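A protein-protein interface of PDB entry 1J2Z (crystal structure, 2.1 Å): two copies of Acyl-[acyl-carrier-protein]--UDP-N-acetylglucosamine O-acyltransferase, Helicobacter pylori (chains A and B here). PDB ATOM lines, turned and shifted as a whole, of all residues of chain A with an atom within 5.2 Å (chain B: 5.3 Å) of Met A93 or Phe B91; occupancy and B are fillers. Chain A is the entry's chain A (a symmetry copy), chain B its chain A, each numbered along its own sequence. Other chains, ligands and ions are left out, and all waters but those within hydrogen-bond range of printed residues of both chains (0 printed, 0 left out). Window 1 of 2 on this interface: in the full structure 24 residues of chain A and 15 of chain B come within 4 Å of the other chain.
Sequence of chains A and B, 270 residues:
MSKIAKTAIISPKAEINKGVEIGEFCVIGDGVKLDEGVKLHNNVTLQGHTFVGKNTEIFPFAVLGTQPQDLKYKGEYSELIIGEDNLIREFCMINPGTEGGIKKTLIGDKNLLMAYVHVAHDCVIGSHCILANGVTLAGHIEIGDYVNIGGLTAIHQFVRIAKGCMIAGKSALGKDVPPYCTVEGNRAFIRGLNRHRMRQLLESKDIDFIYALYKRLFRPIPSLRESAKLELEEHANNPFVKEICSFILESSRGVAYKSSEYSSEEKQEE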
ATOM      1  N   PHE A  61     -25.302  -8.694 -12.451  1.00  0.00           N
ATOM      2  CA  PHE A  61     -25.314  -7.398 -13.103  1.00  0.00           C
ATOM      3  C   PHE A  61     -26.645  -6.902 -13.644  1.00  0.00           C
ATOM      4  O   PHE A  61     -26.679  -6.054 -14.537  1.00  0.00           O
ATOM      5  CB  PHE A  61     -24.252  -7.389 -14.204  1.00  0.00           C
ATOM      6  CG  PHE A  61     -22.877  -7.786 -13.714  1.00  0.00           C
ATOM      7  CD1 PHE A  61     -22.084  -8.658 -14.453  1.00  0.00           C
ATOM      8  CD2 PHE A  61     -22.382  -7.292 -12.509  1.00  0.00           C
ATOM      9  CE1 PHE A  61     -20.815  -9.033 -13.998  1.00  0.00           C
ATOM     10  CE2 PHE A  61     -21.116  -7.659 -12.043  1.00  0.00           C
ATOM     11  CZ  PHE A  61     -20.333  -8.532 -12.788  1.00  0.00           C
ATOM     12  N   ALA A  62     -27.746  -7.426 -13.116  1.00  0.00           N
ATOM     13  CA  ALA A  62     -29.052  -6.940 -13.538  1.00  0.00           C
ATOM     14  C   ALA A  62     -29.296  -5.691 -12.690  1.00  0.00           C
ATOM     15  O   ALA A  62     -28.822  -5.608 -11.556  1.00  0.00           O
ATOM     16  CB  ALA A  62     -30.127  -7.977 -13.253  1.00  0.00           C
ATOM     17  N   VAL A  63     -30.013  -4.716 -13.235  1.00  0.00           N
ATOM     18  CA  VAL A  63     -30.301  -3.500 -12.487  1.00  0.00           C
ATOM     19  C   VAL A  63     -31.801  -3.280 -12.479  1.00  0.00           C
ATOM     20  O   VAL A  63     -32.414  -3.101 -13.533  1.00  0.00           O
ATOM     21  CB  VAL A  63     -29.609  -2.275 -13.121  1.00  0.00           C
ATOM     22  CG1 VAL A  63     -29.985  -1.007 -12.372  1.00  0.00           C
ATOM     23  CG2 VAL A  63     -28.102  -2.470 -13.090  1.00  0.00           C
ATOM     24  N   LEU A  64     -32.392  -3.297 -11.289  1.00  0.00           N
ATOM     25  CA  LEU A  64     -33.833  -3.113 -11.171  1.00  0.00           C
ATOM     26  C   LEU A  64     -34.184  -2.002 -10.196  1.00  0.00           C
ATOM     27  O   LEU A  64     -33.665  -1.946  -9.082  1.00  0.00           O
ATOM     28  CB  LEU A  64     -34.502  -4.403 -10.690  1.00  0.00           C
ATOM     29  CG  LEU A  64     -34.205  -5.739 -11.375  1.00  0.00           C
ATOM     30  CD1 LEU A  64     -35.167  -6.776 -10.823  1.00  0.00           C
ATOM     31  CD2 LEU A  64     -34.358  -5.629 -12.880  1.00  0.00           C
ATOM     32  N   THR A  66     -33.801   1.467 -10.686  1.00  0.00           N
ATOM     33  CA  THR A  66     -33.198   2.786 -10.833  1.00  0.00           C
ATOM     34  C   THR A  66     -34.228   3.648 -11.552  1.00  0.00           C
ATOM     35  O   THR A  66     -35.130   3.126 -12.206  1.00  0.00           O
ATOM     36  CB  THR A  66     -31.881   2.758 -11.656  1.00  0.00           C
ATOM     37  OG1 THR A  66     -32.106   2.096 -12.906  1.00  0.00           O
ATOM     38  CG2 THR A  66     -30.784   2.043 -10.881  1.00  0.00           C
ATOM     39  N   GLN A  69     -35.420   6.519 -17.516  1.00  0.00           N
ATOM     40  CA  GLN A  69     -34.544   7.335 -18.344  1.00  0.00           C
ATOM     41  C   GLN A  69     -35.297   8.558 -18.850  1.00  0.00           C
ATOM     42  O   GLN A  69     -34.701   9.600 -19.121  1.00  0.00           O
ATOM     43  CB  GLN A  69     -34.012   6.502 -19.512  1.00  0.00           C
ATOM     44  CG  GLN A  69     -33.262   5.261 -19.046  1.00  0.00           C
ATOM     45  CD  GLN A  69     -32.584   4.517 -20.177  1.00  0.00           C
ATOM     46  OE1 GLN A  69     -33.238   3.952 -21.054  1.00  0.00           O
ATOM     47  NE2 GLN A  69     -31.261   4.512 -20.159  1.00  0.00           N
ATOM     48  N   PHE A  91     -27.519  -8.385 -17.064  1.00  0.00           N
ATOM     49  CA  PHE A  91     -27.584  -7.072 -17.707  1.00  0.00           C
ATOM     50  C   PHE A  91     -28.966  -6.507 -18.010  1.00  0.00           C
ATOM     51  O   PHE A  91     -29.086  -5.559 -18.793  1.00  0.00           O
ATOM     52  CB  PHE A  91     -26.753  -7.085 -18.992  1.00  0.00           C
ATOM     53  CG  PHE A  91     -25.400  -7.716 -18.825  1.00  0.00           C
ATOM     54  CD1 PHE A  91     -25.054  -8.856 -19.546  1.00  0.00           C
ATOM     55  CD2 PHE A  91     -24.479  -7.183 -17.932  1.00  0.00           C
ATOM     56  CE1 PHE A  91     -23.807  -9.457 -19.377  1.00  0.00           C
ATOM     57  CE2 PHE A  91     -23.229  -7.774 -17.755  1.00  0.00           C
ATOM     58  CZ  PHE A  91     -22.892  -8.916 -18.480  1.00  0.00           C
ATOM     59  N   CYS A  92     -30.009  -7.081 -17.425  1.00  0.00           N
ATOM     60  CA  CYS A  92     -31.346  -6.536 -17.648  1.00  0.00           C
ATOM     61  C   CYS A  92     -31.446  -5.226 -16.884  1.00  0.00           C
ATOM     62  O   CYS A  92     -30.781  -5.041 -15.868  1.00  0.00           O
ATOM     63  CB  CYS A  92     -32.429  -7.490 -17.149  1.00  0.00           C
ATOM     64  SG  CYS A  92     -32.765  -8.845 -18.266  1.00  0.00           S
ATOM     65  N   MET A  93     -32.273  -4.312 -17.378  1.00  0.00           N
ATOM     66  CA  MET A  93     -32.441  -3.022 -16.723  1.00  0.00           C
ATOM     67  C   MET A  93     -33.931  -2.725 -16.746  1.00  0.00           C
ATOM     68  O   MET A  93     -34.531  -2.620 -17.814  1.00  0.00           O
ATOM     69  CB  MET A  93     -31.658  -1.951 -17.482  1.00  0.00           C
ATOM     70  CG  MET A  93     -31.324  -0.705 -16.668  1.00  0.00           C
ATOM     71  SD  MET A  93     -32.629   0.510 -16.685  1.00  0.00           S
ATOM     72  CE  MET A  93     -32.177   1.487 -18.134  1.00  0.00           C
ATOM     73  N   ILE A  94     -34.524  -2.610 -15.563  1.00  0.00           N
ATOM     74  CA  ILE A  94     -35.955  -2.372 -15.442  1.00  0.00           C
ATOM     75  C   ILE A  94     -36.234  -1.185 -14.529  1.00  0.00           C
ATOM     76  O   ILE A  94     -35.779  -1.149 -13.387  1.00  0.00           O
ATOM     77  CB  ILE A  94     -36.657  -3.621 -14.873  1.00  0.00           C
ATOM     78  CG1 ILE A  94     -36.345  -4.833 -15.756  1.00  0.00           C
ATOM     79  CG2 ILE A  94     -38.162  -3.398 -14.810  1.00  0.00           C
ATOM     80  CD1 ILE A  94     -36.928  -6.131 -15.244  1.00  0.00           C
ATOM     81  N   ASN A  95     -36.992  -0.220 -15.038  1.00  0.00           N
ATOM     82  CA  ASN A  95     -37.321   0.975 -14.274  1.00  0.00           C
ATOM     83  C   ASN A  95     -38.755   0.969 -13.771  1.00  0.00           C
ATOM     84  O   ASN A  95     -39.614   0.282 -14.326  1.00  0.00           O
ATOM     85  CB  ASN A  95     -37.118   2.218 -15.144  1.00  0.00           C
ATOM     86  CG  ASN A  95     -35.719   2.305 -15.711  1.00  0.00           C
ATOM     87  OD1 ASN A  95     -34.737   2.291 -14.969  1.00  0.00           O
ATOM     88  ND2 ASN A  95     -35.622   2.394 -17.029  1.00  0.00           N
ATOM     89  N   VAL A 117     -32.097  -7.314 -21.635  1.00  0.00           N
ATOM     90  CA  VAL A 117     -33.476  -6.877 -21.849  1.00  0.00           C
ATOM     91  C   VAL A 117     -33.772  -5.617 -21.032  1.00  0.00           C
ATOM     92  O   VAL A 117     -33.460  -5.550 -19.847  1.00  0.00           O
ATOM     93  CB  VAL A 117     -34.499  -7.974 -21.436  1.00  0.00           C
ATOM     94  CG1 VAL A 117     -35.900  -7.369 -21.313  1.00  0.00           C
ATOM     95  CG2 VAL A 117     -34.511  -9.095 -22.470  1.00  0.00           C
ATOM     96  N   HIS A 118     -34.353  -4.608 -21.671  1.00  0.00           N
ATOM     97  CA  HIS A 118     -34.706  -3.391 -20.949  1.00  0.00           C
ATOM     98  C   HIS A 118     -36.214  -3.188 -20.926  1.00  0.00           C
ATOM     99  O   HIS A 118     -36.868  -3.218 -21.967  1.00  0.00           O
ATOM    100  CB  HIS A 118     -34.067  -2.148 -21.573  1.00  0.00           C
ATOM    101  CG  HIS A 118     -34.578  -0.865 -20.986  1.00  0.00           C
ATOM    102  ND1 HIS A 118     -35.213   0.098 -21.738  1.00  0.00           N
ATOM    103  CD2 HIS A 118     -34.593  -0.415 -19.711  1.00  0.00           C
ATOM    104  CE1 HIS A 118     -35.599   1.087 -20.951  1.00  0.00           C
ATOM    105  NE2 HIS A 118     -35.235   0.799 -19.715  1.00  0.00           N
ATOM    106  N   VAL A 119     -36.759  -2.982 -19.734  1.00  0.00           N
ATOM    107  CA  VAL A 119     -38.187  -2.735 -19.586  1.00  0.00           C
ATOM    108  C   VAL A 119     -38.327  -1.309 -19.070  1.00  0.00           C
ATOM    109  O   VAL A 119     -37.940  -1.007 -17.944  1.00  0.00           O
ATOM    110  CB  VAL A 119     -38.833  -3.717 -18.596  1.00  0.00           C
ATOM    111  CG1 VAL A 119     -40.322  -3.385 -18.427  1.00  0.00           C
ATOM    112  CG2 VAL A 119     -38.668  -5.132 -19.109  1.00  0.00           C
ATOM    113  N   PRO B  60     -25.200   2.625 -12.361  1.00  0.00           N
ATOM    114  CA  PRO B  60     -24.571   1.315 -12.160  1.00  0.00           C
ATOM    115  C   PRO B  60     -24.054   0.550 -13.366  1.00  0.00           C
ATOM    116  O   PRO B  60     -24.684   0.499 -14.418  1.00  0.00           O
ATOM    117  CB  PRO B  60     -25.647   0.523 -11.413  1.00  0.00           C
ATOM    118  CG  PRO B  60     -26.361   1.581 -10.633  1.00  0.00           C
ATOM    119  CD  PRO B  60     -26.496   2.685 -11.655  1.00  0.00           C
ATOM    120  N   PHE B  61     -22.885  -0.052 -13.179  1.00  0.00           N
ATOM    121  CA  PHE B  61     -22.243  -0.882 -14.184  1.00  0.00           C
ATOM    122  C   PHE B  61     -21.805  -0.203 -15.471  1.00  0.00           C
ATOM    123  O   PHE B  61     -21.644  -0.861 -16.500  1.00  0.00           O
ATOM    124  CB  PHE B  61     -23.148  -2.076 -14.489  1.00  0.00           C
ATOM    125  CG  PHE B  61     -23.550  -2.854 -13.256  1.00  0.00           C
ATOM    126  CD1 PHE B  61     -24.862  -3.285 -13.083  1.00  0.00           C
ATOM    127  CD2 PHE B  61     -22.615  -3.148 -12.266  1.00  0.00           C
ATOM    128  CE1 PHE B  61     -25.237  -3.998 -11.940  1.00  0.00           C
ATOM    129  CE2 PHE B  61     -22.978  -3.861 -11.118  1.00  0.00           C
ATOM    130  CZ  PHE B  61     -24.290  -4.284 -10.955  1.00  0.00           C
ATOM    131  N   ALA B  62     -21.616   1.111 -15.429  1.00  0.00           N
ATOM    132  CA  ALA B  62     -21.125   1.810 -16.609  1.00  0.00           C
ATOM    133  C   ALA B  62     -19.606   1.635 -16.561  1.00  0.00           C
ATOM    134  O   ALA B  62     -19.026   1.542 -15.478  1.00  0.00           O
ATOM    135  CB  ALA B  62     -21.479   3.287 -16.543  1.00  0.00           C
ATOM    136  N   VAL B  63     -18.964   1.574 -17.721  1.00  0.00           N
ATOM    137  CA  VAL B  63     -17.517   1.423 -17.759  1.00  0.00           C
ATOM    138  C   VAL B  63     -16.936   2.539 -18.606  1.00  0.00           C
ATOM    139  O   VAL B  63     -17.229   2.638 -19.799  1.00  0.00           O
ATOM    140  CB  VAL B  63     -17.110   0.062 -18.362  1.00  0.00           C
ATOM    141  CG1 VAL B  63     -15.597  -0.043 -18.465  1.00  0.00           C
ATOM    142  CG2 VAL B  63     -17.652  -1.061 -17.490  1.00  0.00           C
ATOM    143  N   ARG B  89     -26.235   6.446 -18.408  1.00  0.00           N
ATOM    144  CA  ARG B  89     -26.941   5.301 -17.854  1.00  0.00           C
ATOM    145  C   ARG B  89     -26.190   3.978 -17.763  1.00  0.00           C
ATOM    146  O   ARG B  89     -25.033   3.859 -18.170  1.00  0.00           O
ATOM    147  CB  ARG B  89     -28.256   5.105 -18.615  1.00  0.00           C
ATOM    148  CG  ARG B  89     -29.194   6.308 -18.512  1.00  0.00           C
ATOM    149  CD  ARG B  89     -29.517   6.660 -17.050  1.00  0.00           C
ATOM    150  NE  ARG B  89     -30.100   5.540 -16.309  1.00  0.00           N
ATOM    151  CZ  ARG B  89     -31.268   5.585 -15.667  1.00  0.00           C
ATOM    152  NH1 ARG B  89     -31.994   6.693 -15.675  1.00  0.00           N
ATOM    153  NH2 ARG B  89     -31.702   4.526 -14.993  1.00  0.00           N
ATOM    154  N   GLU B  90     -26.887   2.991 -17.210  1.00  0.00           N
ATOM    155  CA  GLU B  90     -26.367   1.645 -16.988  1.00  0.00           C
ATOM    156  C   GLU B  90     -25.779   0.927 -18.204  1.00  0.00           C
ATOM    157  O   GLU B  90     -26.324   0.986 -19.304  1.00  0.00           O
ATOM    158  CB  GLU B  90     -27.472   0.760 -16.403  1.00  0.00           C
ATOM    159  CG  GLU B  90     -28.028   1.209 -15.059  1.00  0.00           C
ATOM    160  CD  GLU B  90     -29.097   2.288 -15.163  1.00  0.00           C
ATOM    161  OE1 GLU B  90     -29.773   2.523 -14.145  1.00  0.00           O
ATOM    162  OE2 GLU B  90     -29.266   2.903 -16.241  1.00  0.00           O
ATOM    163  N   PHE B  91     -24.665   0.240 -17.979  1.00  0.00           N
ATOM    164  CA  PHE B  91     -23.991  -0.551 -19.010  1.00  0.00           C
ATOM    165  C   PHE B  91     -23.352   0.204 -20.167  1.00  0.00           C
ATOM    166  O   PHE B  91     -23.026  -0.400 -21.194  1.00  0.00           O
ATOM    167  CB  PHE B  91     -24.956  -1.601 -19.566  1.00  0.00           C
ATOM    168  CG  PHE B  91     -25.717  -2.340 -18.503  1.00  0.00           C
ATOM    169  CD1 PHE B  91     -27.106  -2.266 -18.443  1.00  0.00           C
ATOM    170  CD2 PHE B  91     -25.044  -3.093 -17.549  1.00  0.00           C
ATOM    171  CE1 PHE B  91     -27.814  -2.933 -17.443  1.00  0.00           C
ATOM    172  CE2 PHE B  91     -25.741  -3.765 -16.546  1.00  0.00           C
ATOM    173  CZ  PHE B  91     -27.130  -3.684 -16.493  1.00  0.00           C
ATOM    174  N   CYS B  92     -23.184   1.515 -20.032  1.00  0.00           N
ATOM    175  CA  CYS B  92     -22.525   2.266 -21.097  1.00  0.00           C
ATOM    176  C   CYS B  92     -21.046   1.921 -21.064  1.00  0.00           C
ATOM    177  O   CYS B  92     -20.505   1.585 -20.012  1.00  0.00           O
ATOM    178  CB  CYS B  92     -22.691   3.772 -20.903  1.00  0.00           C
ATOM    179  SG  CYS B  92     -24.288   4.392 -21.415  1.00  0.00           S
ATOM    180  N   MET B  93     -20.393   1.993 -22.217  1.00  0.00           N
ATOM    181  CA  MET B  93     -18.972   1.680 -22.295  1.00  0.00           C
ATOM    182  C   MET B  93     -18.352   2.740 -23.190  1.00  0.00           C
ATOM    183  O   MET B  93     -18.715   2.863 -24.358  1.00  0.00           O
ATOM    184  CB  MET B  93     -18.781   0.285 -22.887  1.00  0.00           C
ATOM    185  CG  MET B  93     -17.441  -0.369 -22.568  1.00  0.00           C
ATOM    186  SD  MET B  93     -16.153   0.084 -23.715  1.00  0.00           S
ATOM    187  CE  MET B  93     -16.338  -1.199 -24.972  1.00  0.00           C
ATOM    188  N   ALA B 115     -28.917   3.510 -21.518  1.00  0.00           N
ATOM    189  CA  ALA B 115     -28.248   2.237 -21.270  1.00  0.00           C
ATOM    190  C   ALA B 115     -27.708   1.515 -22.497  1.00  0.00           C
ATOM    191  O   ALA B 115     -28.239   1.638 -23.600  1.00  0.00           O
ATOM    192  CB  ALA B 115     -29.179   1.309 -20.484  1.00  0.00           C
ATOM    193  N   TYR B 116     -26.637   0.758 -22.275  1.00  0.00           N
ATOM    194  CA  TYR B 116     -25.971  -0.030 -23.305  1.00  0.00           C
ATOM    195  C   TYR B 116     -25.362   0.786 -24.447  1.00  0.00           C
ATOM    196  O   TYR B 116     -25.060   0.236 -25.506  1.00  0.00           O
ATOM    197  CB  TYR B 116     -26.934  -1.074 -23.894  1.00  0.00           C
ATOM    198  CG  TYR B 116     -27.822  -1.767 -22.876  1.00  0.00           C
ATOM    199  CD1 TYR B 116     -29.097  -1.281 -22.603  1.00  0.00           C
ATOM    200  CD2 TYR B 116     -27.394  -2.915 -22.202  1.00  0.00           C
ATOM    201  CE1 TYR B 116     -29.931  -1.911 -21.693  1.00  0.00           C
ATOM    202  CE2 TYR B 116     -28.230  -3.563 -21.279  1.00  0.00           C
ATOM    203  CZ  TYR B 116     -29.501  -3.045 -21.033  1.00  0.00           C
ATOM    204  OH  TYR B 116     -30.347  -3.639 -20.129  1.00  0.00           O
ATOM    205  N   VAL B 117     -25.192   2.090 -24.247  1.00  0.00           N
ATOM    206  CA  VAL B 117     -24.601   2.934 -25.286  1.00  0.00           C
ATOM    207  C   VAL B 117     -23.077   2.788 -25.293  1.00  0.00           C
ATOM    208  O   VAL B 117     -22.436   2.849 -24.248  1.00  0.00           O
ATOM    209  CB  VAL B 117     -24.943   4.435 -25.073  1.00  0.00           C
ATOM    210  CG1 VAL B 117     -24.025   5.314 -25.928  1.00  0.00           C
ATOM    211  CG2 VAL B 117     -26.399   4.699 -25.444  1.00  0.00           C
ATOM    212  N   ASN B 133     -31.075   3.841 -26.058  1.00  0.00           N
ATOM    213  CA  ASN B 133     -30.597   2.494 -25.755  1.00  0.00           C
ATOM    214  C   ASN B 133     -29.819   1.824 -26.877  1.00  0.00           C
ATOM    215  O   ASN B 133     -30.252   1.819 -28.032  1.00  0.00           O
ATOM    216  CB  ASN B 133     -31.764   1.557 -25.383  1.00  0.00           C
ATOM    217  CG  ASN B 133     -32.325   1.820 -23.991  1.00  0.00           C
ATOM    218  OD1 ASN B 133     -32.612   0.887 -23.238  1.00  0.00           O
ATOM    219  ND2 ASN B 133     -32.499   3.083 -23.653  1.00  0.00           N
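Among the printed residues, pairs that only touch across the chains: Phe A61 with Phe B61 (3.6 Å), Phe A61 with Phe B91 (3.1 Å), Ala A62 with Phe B61 (3.9 Å), Val A63 with Phe B61 (3.3 Å), Val A63 with Glu B90 (3.96 Å), Val A63 with Phe B91 (3.7 Å), Gln A69 with Arg B89 (3.2 Å), Phe A91 with Phe B91 (3.2 Å), Cys A92 with Phe B91 (3.9 Å), Cys A92 with Tyr B116 (3.8 Å), Met A93 with Glu B90 (3.7 Å), Met A93 with Phe B91 (3.97 Å), Met A93 with Ala B115 (3.8 Å), Asn A95 with Arg B89 (3.8 Å) and Val A117 with Tyr B116 (3.7 Å).
Met A93 touches four residues of chain B.
Phe B91 touches just these residues of chain A: Phe A61, Val A63, Phe A91, Cys A92 and Met A93.
Printed residues of chain B within 4 Å of Val A63: Phe B61, Glu B90 and Phe B91.
Of the printed residues of chain B, Thr A66 touches Arg B89 (3.2 Å) and Glu B90 (2.7 Å).
Printed residues of chain B within 4 Å of Ala A62: Phe B61 (3.9 Å).
Of the printed residues of chain B, Val A117 touches Tyr B116.
Of the printed residues of chain B, Phe A91 touches Phe B91 and Tyr B116.
Val A119 touches none of the printed residues of chain B.
Ile A94 touches none of the printed residues of chain B.
The nearest residue of chain B that does not touch Met A93 is Arg B89 (4.4 Å).
The nearest residue of chain A that does not touch Phe B91 is Ala A62 (4.8 Å).
The nearest printed residue of chain A that does not touch Arg B89 is Met A93 (4.4 Å).
The guanidinium group (NH2) of Arg B89 lies within hydrogen-bond range of the side-chain hydroxyl (OG1) of Thr A66, 3.2 Å away.
ND2 of Asn B133 sits at hydrogen-bond distance from OE1 of Gln A69 (2.8 Å).
The backbone NH (N) of Met A93 sits close to the side-chain hydroxyl (OH) of Tyr B116, at 3.4 Å.
The backbone NH of Ala B115 lies close to the side-chain amide nitrogen of Gln A69 (2.9 Å).
The backbone carbonyl oxygen (O) of Phe A91 lies within hydrogen-bond range of the side-chain hydroxyl (OH) of Tyr B116 (2.7 Å).
The side-chain hydroxyl (OG1) of Thr A66 is in hydrogen-bond range of the side-chain carboxylate (OE1) of Glu B90, 2.7 Å away.
A ring nitrogen (ND1) of His A118 lies within hydrogen-bond range of the side-chain amide oxygen (OD1) of Asn B133 (3.1 Å).
The backbone carbonyl oxygen of Val A117 lies within hydrogen-bond range of the backbone NH of Met A93.
The side-chain amide oxygen (OD1) of Asn A95 lies close to the side-chain sulfur (SD) of Met A93, at 3.2 Å.
The guanidinium group (NE) of Arg B89 is in salt-bridge range of the side-chain carboxylate (OE2) of Glu B90 (2.8 Å).
The backbone carbonyl oxygen (O) of Met A93 sits at hydrogen-bond distance from the backbone NH (N) of Val A119 (3.0 Å).
The backbone carbonyl oxygen (O) of Cys A92 sits at hydrogen-bond distance from the backbone NH (N) of Val A63, 2.8 Å away.
OD1 of Asn A95 lies close to O of Thr A66, at 2.9 Å.
Hydrophobic or aromatic side chains of chain B that line the printed part of chain A: Phe B61, Phe B91, Ala B115 and Tyr B116.
Of the 14 printed residues of chain A, 11 touch a printed residue of chain B.
Hydrophobic or aromatic side chains of chain A that line the printed part of chain B: Phe A61, Val A63, Phe A91, Met A93 and His A118.
Among the printed residues, 22 pairs touch across the chains.
Among the printed residues, no Asp or Glu carboxylate lies within 4 Å of a Lys or Arg side-chain nitrogen of the other chain.
Phe B61 touches its own counterpart, Phe A61.
Ala A62 touches Phe B61, but with the chains exchanged Phe A61 does not touch Ala B62 (8.8 Å).
Val A63 touches Phe B91, but with the chains exchanged Phe A91 does not touch Val B63 (8.7 Å).
Cys A92 touches Phe B91, but with the chains exchanged Phe A91 does not touch Cys B92 (9.0 Å).
Of the 22 pairs that touch across the chains among the printed residues, 2 have their exchanged pair printed and touching as well.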
